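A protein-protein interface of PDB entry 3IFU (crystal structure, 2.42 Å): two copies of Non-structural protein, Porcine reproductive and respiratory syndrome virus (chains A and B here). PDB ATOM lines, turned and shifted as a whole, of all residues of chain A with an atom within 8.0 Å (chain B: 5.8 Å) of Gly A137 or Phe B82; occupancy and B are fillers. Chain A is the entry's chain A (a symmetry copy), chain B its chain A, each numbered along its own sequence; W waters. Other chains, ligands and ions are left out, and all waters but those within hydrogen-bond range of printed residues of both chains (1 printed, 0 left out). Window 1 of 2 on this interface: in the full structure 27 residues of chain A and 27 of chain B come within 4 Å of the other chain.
Water W1 lies within hydrogen-bond range of the guanidinium group (NH2) of Arg B86 and the backbone carbonyl oxygen (O) of Asn A161.
Gly A137 touches one residue of chain B.
Printed residues of chain B within 4 Å of Lys A150: Glu B20 (3.2 Å).
Printed residues of chain A within 4 Å of Ala B19: Pro A136 (3.9 Å).
Ser B79 touches none of the printed residues of chain A.
OG1 of Thr A160 is in hydrogen-bond range of N of Leu A162, at 3.1 Å.
3 positions are printed for both chains.
Of the 8 pairs that touch across the chains among the printed residues, none has its exchanged pair printed and touching as well.
Printed residues of chain A that touch a printed residue of chain B: Pro A136, Gly A137, Lys A150, Asn A161, Leu A162 and Pro A163.
Printed residues of chain B that touch a printed residue of chain A: Ala B19, Glu B20, Leu B29, Phe B82, Arg B86 and Phe B94.
Hydrophobic or aromatic side chains of chain B that line the printed part of chain A: Ala B19, Leu B29, Phe B82 and Phe B94.
Among the printed residues, 8 pairs touch across the chains.
Among the printed residues, pairs that only touch across the chains: Pro A136 with Ala B19 (3.9 Å), Gly A137 with Phe B82 (3.5 Å), Lys A150 with Glu B20 (3.2 Å), Asn A161 with Arg B86 (3.7 Å), Leu A162 with Arg B86 (3.99 Å), Leu A162 with Phe B94 (3.7 Å), Pro A163 with Leu B29 (3.6 Å) and Pro A163 with Phe B94 (3.7 Å).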
ATOM      1  N   PRO A  83       7.884   8.823 -29.521  1.00  0.00           N
ATOM      2  CA  PRO A  83       7.949   8.508 -28.087  1.00  0.00           C
ATOM      3  C   PRO A  83       8.636   9.587 -27.243  1.00  0.00           C
ATOM      4  O   PRO A  83       8.168   9.922 -26.152  1.00  0.00           O
ATOM      5  CB  PRO A  83       8.708   7.188 -28.058  1.00  0.00           C
ATOM      6  CG  PRO A  83       8.292   6.557 -29.325  1.00  0.00           C
ATOM      7  CD  PRO A  83       8.382   7.688 -30.316  1.00  0.00           C
ATOM      8  N   MET A  87       6.438  11.668 -24.363  1.00  0.00           N
ATOM      9  CA  MET A  87       6.838  11.569 -22.965  1.00  0.00           C
ATOM     10  C   MET A  87       7.432  12.870 -22.458  1.00  0.00           C
ATOM     11  O   MET A  87       7.583  13.070 -21.260  1.00  0.00           O
ATOM     12  CB  MET A  87       7.864  10.451 -22.793  1.00  0.00           C
ATOM     13  CG  MET A  87       7.467   9.140 -23.450  1.00  0.00           C
ATOM     14  SD  MET A  87       8.551   7.758 -23.042  1.00  0.00           S
ATOM     15  CE  MET A  87       9.898   8.012 -24.159  1.00  0.00           C
ATOM     16  N   PRO A 134       7.600  -6.953 -19.767  1.00  0.00           N
ATOM     17  CA  PRO A 134       6.767  -6.062 -20.576  1.00  0.00           C
ATOM     18  C   PRO A 134       6.527  -4.687 -19.955  1.00  0.00           C
ATOM     19  O   PRO A 134       6.363  -4.557 -18.750  1.00  0.00           O
ATOM     20  CB  PRO A 134       5.454  -6.842 -20.718  1.00  0.00           C
ATOM     21  CG  PRO A 134       5.817  -8.260 -20.369  1.00  0.00           C
ATOM     22  CD  PRO A 134       6.813  -8.093 -19.273  1.00  0.00           C
ATOM     23  N   VAL A 135       6.515  -3.658 -20.795  1.00  0.00           N
ATOM     24  CA  VAL A 135       6.247  -2.299 -20.336  1.00  0.00           C
ATOM     25  C   VAL A 135       5.095  -1.748 -21.162  1.00  0.00           C
ATOM     26  O   VAL A 135       5.135  -1.765 -22.392  1.00  0.00           O
ATOM     27  CB  VAL A 135       7.454  -1.365 -20.512  1.00  0.00           C
ATOM     28  CG1 VAL A 135       7.057   0.073 -20.118  1.00  0.00           C
ATOM     29  CG2 VAL A 135       8.609  -1.848 -19.651  1.00  0.00           C
ATOM     30  N   PRO A 136       4.048  -1.254 -20.494  1.00  0.00           N
ATOM     31  CA  PRO A 136       2.900  -0.708 -21.225  1.00  0.00           C
ATOM     32  C   PRO A 136       3.152   0.701 -21.754  1.00  0.00           C
ATOM     33  O   PRO A 136       4.035   1.412 -21.271  1.00  0.00           O
ATOM     34  CB  PRO A 136       1.801  -0.737 -20.179  1.00  0.00           C
ATOM     35  CG  PRO A 136       2.563  -0.366 -18.926  1.00  0.00           C
ATOM     36  CD  PRO A 136       3.828  -1.199 -19.036  1.00  0.00           C
ATOM     37  N   GLY A 137       2.378   1.090 -22.761  1.00  0.00           N
ATOM     38  CA  GLY A 137       2.501   2.422 -23.312  1.00  0.00           C
ATOM     39  C   GLY A 137       3.667   2.695 -24.234  1.00  0.00           C
ATOM     40  O   GLY A 137       4.339   1.787 -24.704  1.00  0.00           O
ATOM     41  N   VAL A 138       3.901   3.980 -24.470  1.00  0.00           N
ATOM     42  CA  VAL A 138       4.953   4.448 -25.353  1.00  0.00           C
ATOM     43  C   VAL A 138       6.346   4.412 -24.732  1.00  0.00           C
ATOM     44  O   VAL A 138       6.513   4.582 -23.522  1.00  0.00           O
ATOM     45  CB  VAL A 138       4.665   5.884 -25.808  1.00  0.00           C
ATOM     46  CG1 VAL A 138       3.369   5.933 -26.600  1.00  0.00           C
ATOM     47  CG2 VAL A 138       4.579   6.787 -24.593  1.00  0.00           C
ATOM     48  N   GLY A 139       7.351   4.191 -25.570  1.00  0.00           N
ATOM     49  CA  GLY A 139       8.707   4.153 -25.070  1.00  0.00           C
ATOM     50  C   GLY A 139       9.726   3.965 -26.168  1.00  0.00           C
ATOM     51  O   GLY A 139       9.395   3.745 -27.331  1.00  0.00           O
ATOM     52  N   VAL A 140      10.987   4.083 -25.793  1.00  0.00           N
ATOM     53  CA  VAL A 140      12.060   3.893 -26.741  1.00  0.00           C
ATOM     54  C   VAL A 140      12.850   2.704 -26.232  1.00  0.00           C
ATOM     55  O   VAL A 140      13.391   2.734 -25.137  1.00  0.00           O
ATOM     56  CB  VAL A 140      12.975   5.139 -26.825  1.00  0.00           C
ATOM     57  CG1 VAL A 140      14.062   4.919 -27.870  1.00  0.00           C
ATOM     58  CG2 VAL A 140      12.148   6.363 -27.185  1.00  0.00           C
ATOM     59  N   TYR A 141      12.870   1.638 -27.021  1.00  0.00           N
ATOM     60  CA  TYR A 141      13.606   0.438 -26.662  1.00  0.00           C
ATOM     61  C   TYR A 141      14.946   0.572 -27.330  1.00  0.00           C
ATOM     62  O   TYR A 141      15.032   1.127 -28.419  1.00  0.00           O
ATOM     63  CB  TYR A 141      12.854  -0.790 -27.158  1.00  0.00           C
ATOM     64  CG  TYR A 141      11.566  -0.976 -26.401  1.00  0.00           C
ATOM     65  CD1 TYR A 141      11.483  -1.882 -25.349  1.00  0.00           C
ATOM     66  CD2 TYR A 141      10.451  -0.178 -26.678  1.00  0.00           C
ATOM     67  CE1 TYR A 141      10.326  -1.989 -24.583  1.00  0.00           C
ATOM     68  CE2 TYR A 141       9.288  -0.278 -25.917  1.00  0.00           C
ATOM     69  CZ  TYR A 141       9.233  -1.184 -24.869  1.00  0.00           C
ATOM     70  OH  TYR A 141       8.103  -1.275 -24.090  1.00  0.00           O
ATOM     71  N   ASP A 149      10.507   2.083 -31.178  1.00  0.00           N
ATOM     72  CA  ASP A 149       9.391   2.491 -30.336  1.00  0.00           C
ATOM     73  C   ASP A 149       8.684   1.252 -29.781  1.00  0.00           C
ATOM     74  O   ASP A 149       7.727   1.341 -29.016  1.00  0.00           O
ATOM     75  CB  ASP A 149       8.428   3.381 -31.134  1.00  0.00           C
ATOM     76  CG  ASP A 149       7.697   2.632 -32.228  1.00  0.00           C
ATOM     77  OD1 ASP A 149       8.342   1.897 -33.007  1.00  0.00           O
ATOM     78  OD2 ASP A 149       6.464   2.792 -32.314  1.00  0.00           O
ATOM     79  N   LYS A 150       9.189   0.088 -30.165  1.00  0.00           N
ATOM     80  CA  LYS A 150       8.641  -1.184 -29.710  1.00  0.00           C
ATOM     81  C   LYS A 150       9.794  -2.129 -29.373  1.00  0.00           C
ATOM     82  O   LYS A 150      10.907  -1.959 -29.865  1.00  0.00           O
ATOM     83  CB  LYS A 150       7.748  -1.795 -30.796  1.00  0.00           C
ATOM     84  CG  LYS A 150       6.365  -1.156 -30.899  1.00  0.00           C
ATOM     85  CD  LYS A 150       5.508  -1.523 -29.687  1.00  0.00           C
ATOM     86  CE  LYS A 150       4.070  -1.031 -29.811  1.00  0.00           C
ATOM     87  NZ  LYS A 150       3.978   0.457 -29.764  1.00  0.00           N
ATOM     88  N   PRO A 151       9.543  -3.125 -28.511  1.00  0.00           N
ATOM     89  CA  PRO A 151      10.576  -4.088 -28.121  1.00  0.00           C
ATOM     90  C   PRO A 151      11.094  -4.844 -29.335  1.00  0.00           C
ATOM     91  O   PRO A 151      10.383  -4.990 -30.329  1.00  0.00           O
ATOM     92  CB  PRO A 151       9.836  -5.015 -27.160  1.00  0.00           C
ATOM     93  CG  PRO A 151       8.770  -4.147 -26.596  1.00  0.00           C
ATOM     94  CD  PRO A 151       8.282  -3.412 -27.812  1.00  0.00           C
ATOM     95  N   VAL A 158      14.871   0.350 -21.876  1.00  0.00           N
ATOM     96  CA  VAL A 158      13.666   1.040 -22.300  1.00  0.00           C
ATOM     97  C   VAL A 158      13.600   2.395 -21.611  1.00  0.00           C
ATOM     98  O   VAL A 158      13.767   2.499 -20.400  1.00  0.00           O
ATOM     99  CB  VAL A 158      12.402   0.229 -21.967  1.00  0.00           C
ATOM    100  CG1 VAL A 158      12.314  -0.012 -20.471  1.00  0.00           C
ATOM    101  CG2 VAL A 158      11.165   0.959 -22.483  1.00  0.00           C
ATOM    102  N   LEU A 159      13.376   3.432 -22.409  1.00  0.00           N
ATOM    103  CA  LEU A 159      13.281   4.801 -21.920  1.00  0.00           C
ATOM    104  C   LEU A 159      11.804   5.129 -21.732  1.00  0.00           C
ATOM    105  O   LEU A 159      11.026   5.116 -22.695  1.00  0.00           O
ATOM    106  CB  LEU A 159      13.902   5.753 -22.942  1.00  0.00           C
ATOM    107  CG  LEU A 159      13.836   7.258 -22.689  1.00  0.00           C
ATOM    108  CD1 LEU A 159      14.661   7.617 -21.469  1.00  0.00           C
ATOM    109  CD2 LEU A 159      14.353   8.000 -23.921  1.00  0.00           C
ATOM    110  N   THR A 160      11.405   5.413 -20.497  1.00  0.00           N
ATOM    111  CA  THR A 160      10.010   5.735 -20.249  1.00  0.00           C
ATOM    112  C   THR A 160       9.828   6.754 -19.137  1.00  0.00           C
ATOM    113  O   THR A 160      10.683   6.913 -18.271  1.00  0.00           O
ATOM    114  CB  THR A 160       9.202   4.467 -19.901  1.00  0.00           C
ATOM    115  OG1 THR A 160       7.814   4.798 -19.780  1.00  0.00           O
ATOM    116  CG2 THR A 160       9.692   3.866 -18.590  1.00  0.00           C
ATOM    117  N   ASN A 161       8.700   7.447 -19.175  1.00  0.00           N
ATOM    118  CA  ASN A 161       8.391   8.443 -18.163  1.00  0.00           C
ATOM    119  C   ASN A 161       7.421   7.833 -17.168  1.00  0.00           C
ATOM    120  O   ASN A 161       6.924   8.505 -16.276  1.00  0.00           O
ATOM    121  CB  ASN A 161       7.778   9.699 -18.799  1.00  0.00           C
ATOM    122  CG  ASN A 161       6.446   9.430 -19.481  1.00  0.00           C
ATOM    123  OD1 ASN A 161       5.747  10.362 -19.876  1.00  0.00           O
ATOM    124  ND2 ASN A 161       6.095   8.158 -19.631  1.00  0.00           N
ATOM    125  N   LEU A 162       7.167   6.545 -17.337  1.00  0.00           N
ATOM    126  CA  LEU A 162       6.265   5.797 -16.477  1.00  0.00           C
ATOM    127  C   LEU A 162       6.967   5.471 -15.148  1.00  0.00           C
ATOM    128  O   LEU A 162       8.140   5.090 -15.134  1.00  0.00           O
ATOM    129  CB  LEU A 162       5.866   4.512 -17.209  1.00  0.00           C
ATOM    130  CG  LEU A 162       4.468   3.906 -17.151  1.00  0.00           C
ATOM    131  CD1 LEU A 162       3.403   4.956 -17.405  1.00  0.00           C
ATOM    132  CD2 LEU A 162       4.385   2.813 -18.198  1.00  0.00           C
ATOM    133  N   PRO A 163       6.270   5.640 -14.011  1.00  0.00           N
ATOM    134  CA  PRO A 163       6.881   5.344 -12.705  1.00  0.00           C
ATOM    135  C   PRO A 163       7.061   3.838 -12.463  1.00  0.00           C
ATOM    136  O   PRO A 163       6.381   3.248 -11.623  1.00  0.00           O
ATOM    137  CB  PRO A 163       5.907   5.984 -11.719  1.00  0.00           C
ATOM    138  CG  PRO A 163       4.593   5.889 -12.431  1.00  0.00           C
ATOM    139  CD  PRO A 163       4.946   6.265 -13.846  1.00  0.00           C
ATOM    140  N   PHE B  17      -5.241  -4.351 -15.382  1.00  0.00           N
ATOM    141  CA  PHE B  17      -5.639  -3.667 -16.610  1.00  0.00           C
ATOM    142  C   PHE B  17      -4.977  -4.395 -17.772  1.00  0.00           C
ATOM    143  O   PHE B  17      -4.034  -5.151 -17.570  1.00  0.00           O
ATOM    144  CB  PHE B  17      -5.247  -2.175 -16.576  1.00  0.00           C
ATOM    145  CG  PHE B  17      -3.759  -1.906 -16.603  1.00  0.00           C
ATOM    146  CD1 PHE B  17      -3.064  -1.838 -17.813  1.00  0.00           C
ATOM    147  CD2 PHE B  17      -3.062  -1.652 -15.414  1.00  0.00           C
ATOM    148  CE1 PHE B  17      -1.694  -1.515 -17.838  1.00  0.00           C
ATOM    149  CE2 PHE B  17      -1.700  -1.330 -15.429  1.00  0.00           C
ATOM    150  CZ  PHE B  17      -1.016  -1.259 -16.644  1.00  0.00           C
ATOM    151  N   VAL B  18      -5.485  -4.197 -18.981  1.00  0.00           N
ATOM    152  CA  VAL B  18      -4.921  -4.860 -20.150  1.00  0.00           C
ATOM    153  C   VAL B  18      -4.399  -3.861 -21.184  1.00  0.00           C
ATOM    154  O   VAL B  18      -5.119  -2.957 -21.613  1.00  0.00           O
ATOM    155  CB  VAL B  18      -5.972  -5.780 -20.803  1.00  0.00           C
ATOM    156  CG1 VAL B  18      -5.339  -6.625 -21.886  1.00  0.00           C
ATOM    157  CG2 VAL B  18      -6.594  -6.660 -19.751  1.00  0.00           C
ATOM    158  N   ALA B  19      -3.129  -4.022 -21.558  1.00  0.00           N
ATOM    159  CA  ALA B  19      -2.466  -3.168 -22.550  1.00  0.00           C
ATOM    160  C   ALA B  19      -1.940  -4.123 -23.613  1.00  0.00           C
ATOM    161  O   ALA B  19      -1.227  -5.082 -23.306  1.00  0.00           O
ATOM    162  CB  ALA B  19      -1.327  -2.392 -21.915  1.00  0.00           C
ATOM    163  N   GLU B  20      -2.296  -3.856 -24.866  1.00  0.00           N
ATOM    164  CA  GLU B  20      -1.925  -4.735 -25.963  1.00  0.00           C
ATOM    165  C   GLU B  20      -2.260  -6.159 -25.507  1.00  0.00           C
ATOM    166  O   GLU B  20      -3.396  -6.428 -25.121  1.00  0.00           O
ATOM    167  CB  GLU B  20      -0.446  -4.564 -26.325  1.00  0.00           C
ATOM    168  CG  GLU B  20      -0.158  -3.182 -26.919  1.00  0.00           C
ATOM    169  CD  GLU B  20       0.994  -3.168 -27.919  1.00  0.00           C
ATOM    170  OE1 GLU B  20       0.969  -3.979 -28.868  1.00  0.00           O
ATOM    171  OE2 GLU B  20       1.914  -2.336 -27.767  1.00  0.00           O
ATOM    172  N   LEU B  29       2.512  -1.707 -12.035  1.00  0.00           N
ATOM    173  CA  LEU B  29       2.687  -1.627 -13.484  1.00  0.00           C
ATOM    174  C   LEU B  29       3.546  -2.752 -14.067  1.00  0.00           C
ATOM    175  O   LEU B  29       4.090  -2.623 -15.165  1.00  0.00           O
ATOM    176  CB  LEU B  29       3.289  -0.269 -13.851  1.00  0.00           C
ATOM    177  CG  LEU B  29       2.547   0.920 -13.234  1.00  0.00           C
ATOM    178  CD1 LEU B  29       3.356   2.206 -13.371  1.00  0.00           C
ATOM    179  CD2 LEU B  29       1.191   1.045 -13.903  1.00  0.00           C
ATOM    180  N   LEU B  78     -11.417  -3.212 -19.460  1.00  0.00           N
ATOM    181  CA  LEU B  78     -10.159  -3.468 -18.761  1.00  0.00           C
ATOM    182  C   LEU B  78      -9.019  -2.978 -19.641  1.00  0.00           C
ATOM    183  O   LEU B  78      -7.906  -2.705 -19.170  1.00  0.00           O
ATOM    184  CB  LEU B  78      -9.985  -4.966 -18.483  1.00  0.00           C
ATOM    185  CG  LEU B  78     -10.712  -5.549 -17.271  1.00  0.00           C
ATOM    186  CD1 LEU B  78     -10.524  -7.050 -17.232  1.00  0.00           C
ATOM    187  CD2 LEU B  78     -10.164  -4.921 -16.009  1.00  0.00           C
ATOM    188  N   SER B  79      -9.324  -2.870 -20.928  1.00  0.00           N
ATOM    189  CA  SER B  79      -8.379  -2.419 -21.934  1.00  0.00           C
ATOM    190  C   SER B  79      -8.332  -0.887 -22.052  1.00  0.00           C
ATOM    191  O   SER B  79      -7.403  -0.338 -22.632  1.00  0.00           O
ATOM    192  CB  SER B  79      -8.766  -3.055 -23.272  1.00  0.00           C
ATOM    193  OG  SER B  79      -8.026  -2.514 -24.343  1.00  0.00           O
ATOM    194  N   ALA B  80      -9.324  -0.194 -21.494  1.00  0.00           N
ATOM    195  CA  ALA B  80      -9.362   1.264 -21.569  1.00  0.00           C
ATOM    196  C   ALA B  80      -8.752   1.961 -20.351  1.00  0.00           C
ATOM    197  O   ALA B  80      -8.491   3.171 -20.388  1.00  0.00           O
ATOM    198  CB  ALA B  80     -10.792   1.734 -21.771  1.00  0.00           C
ATOM    199  N   ILE B  81      -8.503   1.198 -19.288  1.00  0.00           N
ATOM    200  CA  ILE B  81      -7.938   1.758 -18.064  1.00  0.00           C
ATOM    201  C   ILE B  81      -6.609   2.514 -18.243  1.00  0.00           C
ATOM    202  O   ILE B  81      -6.494   3.678 -17.840  1.00  0.00           O
ATOM    203  CB  ILE B  81      -7.776   0.664 -16.975  1.00  0.00           C
ATOM    204  CG1 ILE B  81      -9.137   0.006 -16.709  1.00  0.00           C
ATOM    205  CG2 ILE B  81      -7.242   1.279 -15.690  1.00  0.00           C
ATOM    206  CD1 ILE B  81      -9.176  -0.889 -15.509  1.00  0.00           C
ATOM    207  N   PHE B  82      -5.618   1.871 -18.854  1.00  0.00           N
ATOM    208  CA  PHE B  82      -4.328   2.512 -19.066  1.00  0.00           C
ATOM    209  C   PHE B  82      -4.374   3.745 -19.984  1.00  0.00           C
ATOM    210  O   PHE B  82      -3.854   4.801 -19.623  1.00  0.00           O
ATOM    211  CB  PHE B  82      -3.303   1.509 -19.612  1.00  0.00           C
ATOM    212  CG  PHE B  82      -1.957   2.112 -19.862  1.00  0.00           C
ATOM    213  CD1 PHE B  82      -1.146   2.497 -18.799  1.00  0.00           C
ATOM    214  CD2 PHE B  82      -1.530   2.375 -21.157  1.00  0.00           C
ATOM    215  CE1 PHE B  82       0.070   3.146 -19.021  1.00  0.00           C
ATOM    216  CE2 PHE B  82      -0.317   3.022 -21.388  1.00  0.00           C
ATOM    217  CZ  PHE B  82       0.482   3.409 -20.313  1.00  0.00           C
ATOM    218  N   PRO B  83      -4.971   3.631 -21.188  1.00  0.00           N
ATOM    219  CA  PRO B  83      -5.030   4.793 -22.085  1.00  0.00           C
ATOM    220  C   PRO B  83      -5.703   6.023 -21.468  1.00  0.00           C
ATOM    221  O   PRO B  83      -5.226   7.149 -21.635  1.00  0.00           O
ATOM    222  CB  PRO B  83      -5.802   4.261 -23.286  1.00  0.00           C
ATOM    223  CG  PRO B  83      -5.399   2.842 -23.316  1.00  0.00           C
ATOM    224  CD  PRO B  83      -5.484   2.431 -21.870  1.00  0.00           C
ATOM    225  N   ILE B  84      -6.814   5.813 -20.767  1.00  0.00           N
ATOM    226  CA  ILE B  84      -7.516   6.929 -20.132  1.00  0.00           C
ATOM    227  C   ILE B  84      -6.643   7.552 -19.042  1.00  0.00           C
ATOM    228  O   ILE B  84      -6.597   8.768 -18.896  1.00  0.00           O
ATOM    229  CB  ILE B  84      -8.867   6.484 -19.511  1.00  0.00           C
ATOM    230  CG1 ILE B  84      -9.856   6.117 -20.620  1.00  0.00           C
ATOM    231  CG2 ILE B  84      -9.425   7.593 -18.642  1.00  0.00           C
ATOM    232  CD1 ILE B  84     -11.102   5.414 -20.132  1.00  0.00           C
ATOM    233  N   ALA B  85      -5.945   6.719 -18.285  1.00  0.00           N
ATOM    234  CA  ALA B  85      -5.079   7.231 -17.239  1.00  0.00           C
ATOM    235  C   ALA B  85      -3.870   7.974 -17.815  1.00  0.00           C
ATOM    236  O   ALA B  85      -3.508   9.040 -17.318  1.00  0.00           O
ATOM    237  CB  ALA B  85      -4.618   6.096 -16.335  1.00  0.00           C
ATOM    238  N   ARG B  86      -3.244   7.432 -18.858  1.00  0.00           N
ATOM    239  CA  ARG B  86      -2.078   8.103 -19.424  1.00  0.00           C
ATOM    240  C   ARG B  86      -2.384   9.440 -20.071  1.00  0.00           C
ATOM    241  O   ARG B  86      -1.636  10.398 -19.897  1.00  0.00           O
ATOM    242  CB  ARG B  86      -1.367   7.248 -20.470  1.00  0.00           C
ATOM    243  CG  ARG B  86       0.029   7.792 -20.776  1.00  0.00           C
ATOM    244  CD  ARG B  86       1.018   7.252 -19.751  1.00  0.00           C
ATOM    245  NE  ARG B  86       1.963   8.220 -19.184  1.00  0.00           N
ATOM    246  CZ  ARG B  86       1.619   9.334 -18.545  1.00  0.00           C
ATOM    247  NH1 ARG B  86       0.342   9.657 -18.398  1.00  0.00           N
ATOM    248  NH2 ARG B  86       2.551  10.100 -17.998  1.00  0.00           N
ATOM    249  N   MET B  87      -3.470   9.498 -20.833  1.00  0.00           N
ATOM    250  CA  MET B  87      -3.862  10.722 -21.519  1.00  0.00           C
ATOM    251  C   MET B  87      -4.442  11.742 -20.557  1.00  0.00           C
ATOM    252  O   MET B  87      -4.584  12.912 -20.889  1.00  0.00           O
ATOM    253  CB  MET B  87      -4.898  10.408 -22.597  1.00  0.00           C
ATOM    254  CG  MET B  87      -4.516   9.249 -23.502  1.00  0.00           C
ATOM    255  SD  MET B  87      -5.611   9.037 -24.921  1.00  0.00           S
ATOM    256  CE  MET B  87      -6.962   8.148 -24.204  1.00  0.00           C
ATOM    257  N   PHE B  94       0.905  10.304 -12.635  1.00  0.00           N
ATOM    258  CA  PHE B  94       0.390   9.054 -13.196  1.00  0.00           C
ATOM    259  C   PHE B  94      -0.101   7.948 -12.257  1.00  0.00           C
ATOM    260  O   PHE B  94      -1.194   7.423 -12.459  1.00  0.00           O
ATOM    261  CB  PHE B  94       1.411   8.433 -14.152  1.00  0.00           C
ATOM    262  CG  PHE B  94       0.920   7.175 -14.807  1.00  0.00           C
ATOM    263  CD1 PHE B  94       0.046   7.239 -15.886  1.00  0.00           C
ATOM    264  CD2 PHE B  94       1.277   5.927 -14.302  1.00  0.00           C
ATOM    265  CE1 PHE B  94      -0.465   6.091 -16.451  1.00  0.00           C
ATOM    266  CE2 PHE B  94       0.766   4.762 -14.866  1.00  0.00           C
ATOM    267  CZ  PHE B  94      -0.109   4.846 -15.942  1.00  0.00           C
ATOM    268  N   MET B  98      -3.766   6.424 -12.296  1.00  0.00           N
ATOM    269  CA  MET B  98      -4.019   5.031 -12.657  1.00  0.00           C
ATOM    270  C   MET B  98      -4.915   4.369 -11.624  1.00  0.00           C
ATOM    271  O   MET B  98      -5.888   3.689 -11.965  1.00  0.00           O
ATOM    272  CB  MET B  98      -2.697   4.266 -12.766  1.00  0.00           C
ATOM    273  CG  MET B  98      -2.820   2.731 -12.808  1.00  0.00           C
ATOM    274  SD  MET B  98      -3.914   2.013 -14.087  1.00  0.00           S
ATOM    275  CE  MET B  98      -3.038   2.363 -15.581  1.00  0.00           C
ATOM    276  N   VAL B 101      -8.576   5.850 -11.722  1.00  0.00           N
ATOM    277  CA  VAL B 101      -9.245   5.437 -12.953  1.00  0.00           C
ATOM    278  C   VAL B 101      -9.709   3.973 -12.893  1.00  0.00           C
ATOM    279  O   VAL B 101     -10.821   3.650 -13.315  1.00  0.00           O
ATOM    280  CB  VAL B 101      -8.312   5.615 -14.160  1.00  0.00           C
ATOM    281  CG1 VAL B 101      -8.917   4.965 -15.394  1.00  0.00           C
ATOM    282  CG2 VAL B 101      -8.070   7.086 -14.402  1.00  0.00           C
ATOM    283  N   VAL B 138      -1.004   6.086 -27.750  1.00  0.00           N
ATOM    284  CA  VAL B 138      -2.056   5.498 -26.943  1.00  0.00           C
ATOM    285  C   VAL B 138      -3.446   6.057 -27.233  1.00  0.00           C
ATOM    286  O   VAL B 138      -3.605   7.225 -27.596  1.00  0.00           O
ATOM    287  CB  VAL B 138      -1.758   5.699 -25.452  1.00  0.00           C
ATOM    288  CG1 VAL B 138      -0.466   4.993 -25.076  1.00  0.00           C
ATOM    289  CG2 VAL B 138      -1.657   7.183 -25.156  1.00  0.00           C
HETATM  290  O   HOH W   1       4.413   9.703 -16.043  1.00  0.00           O
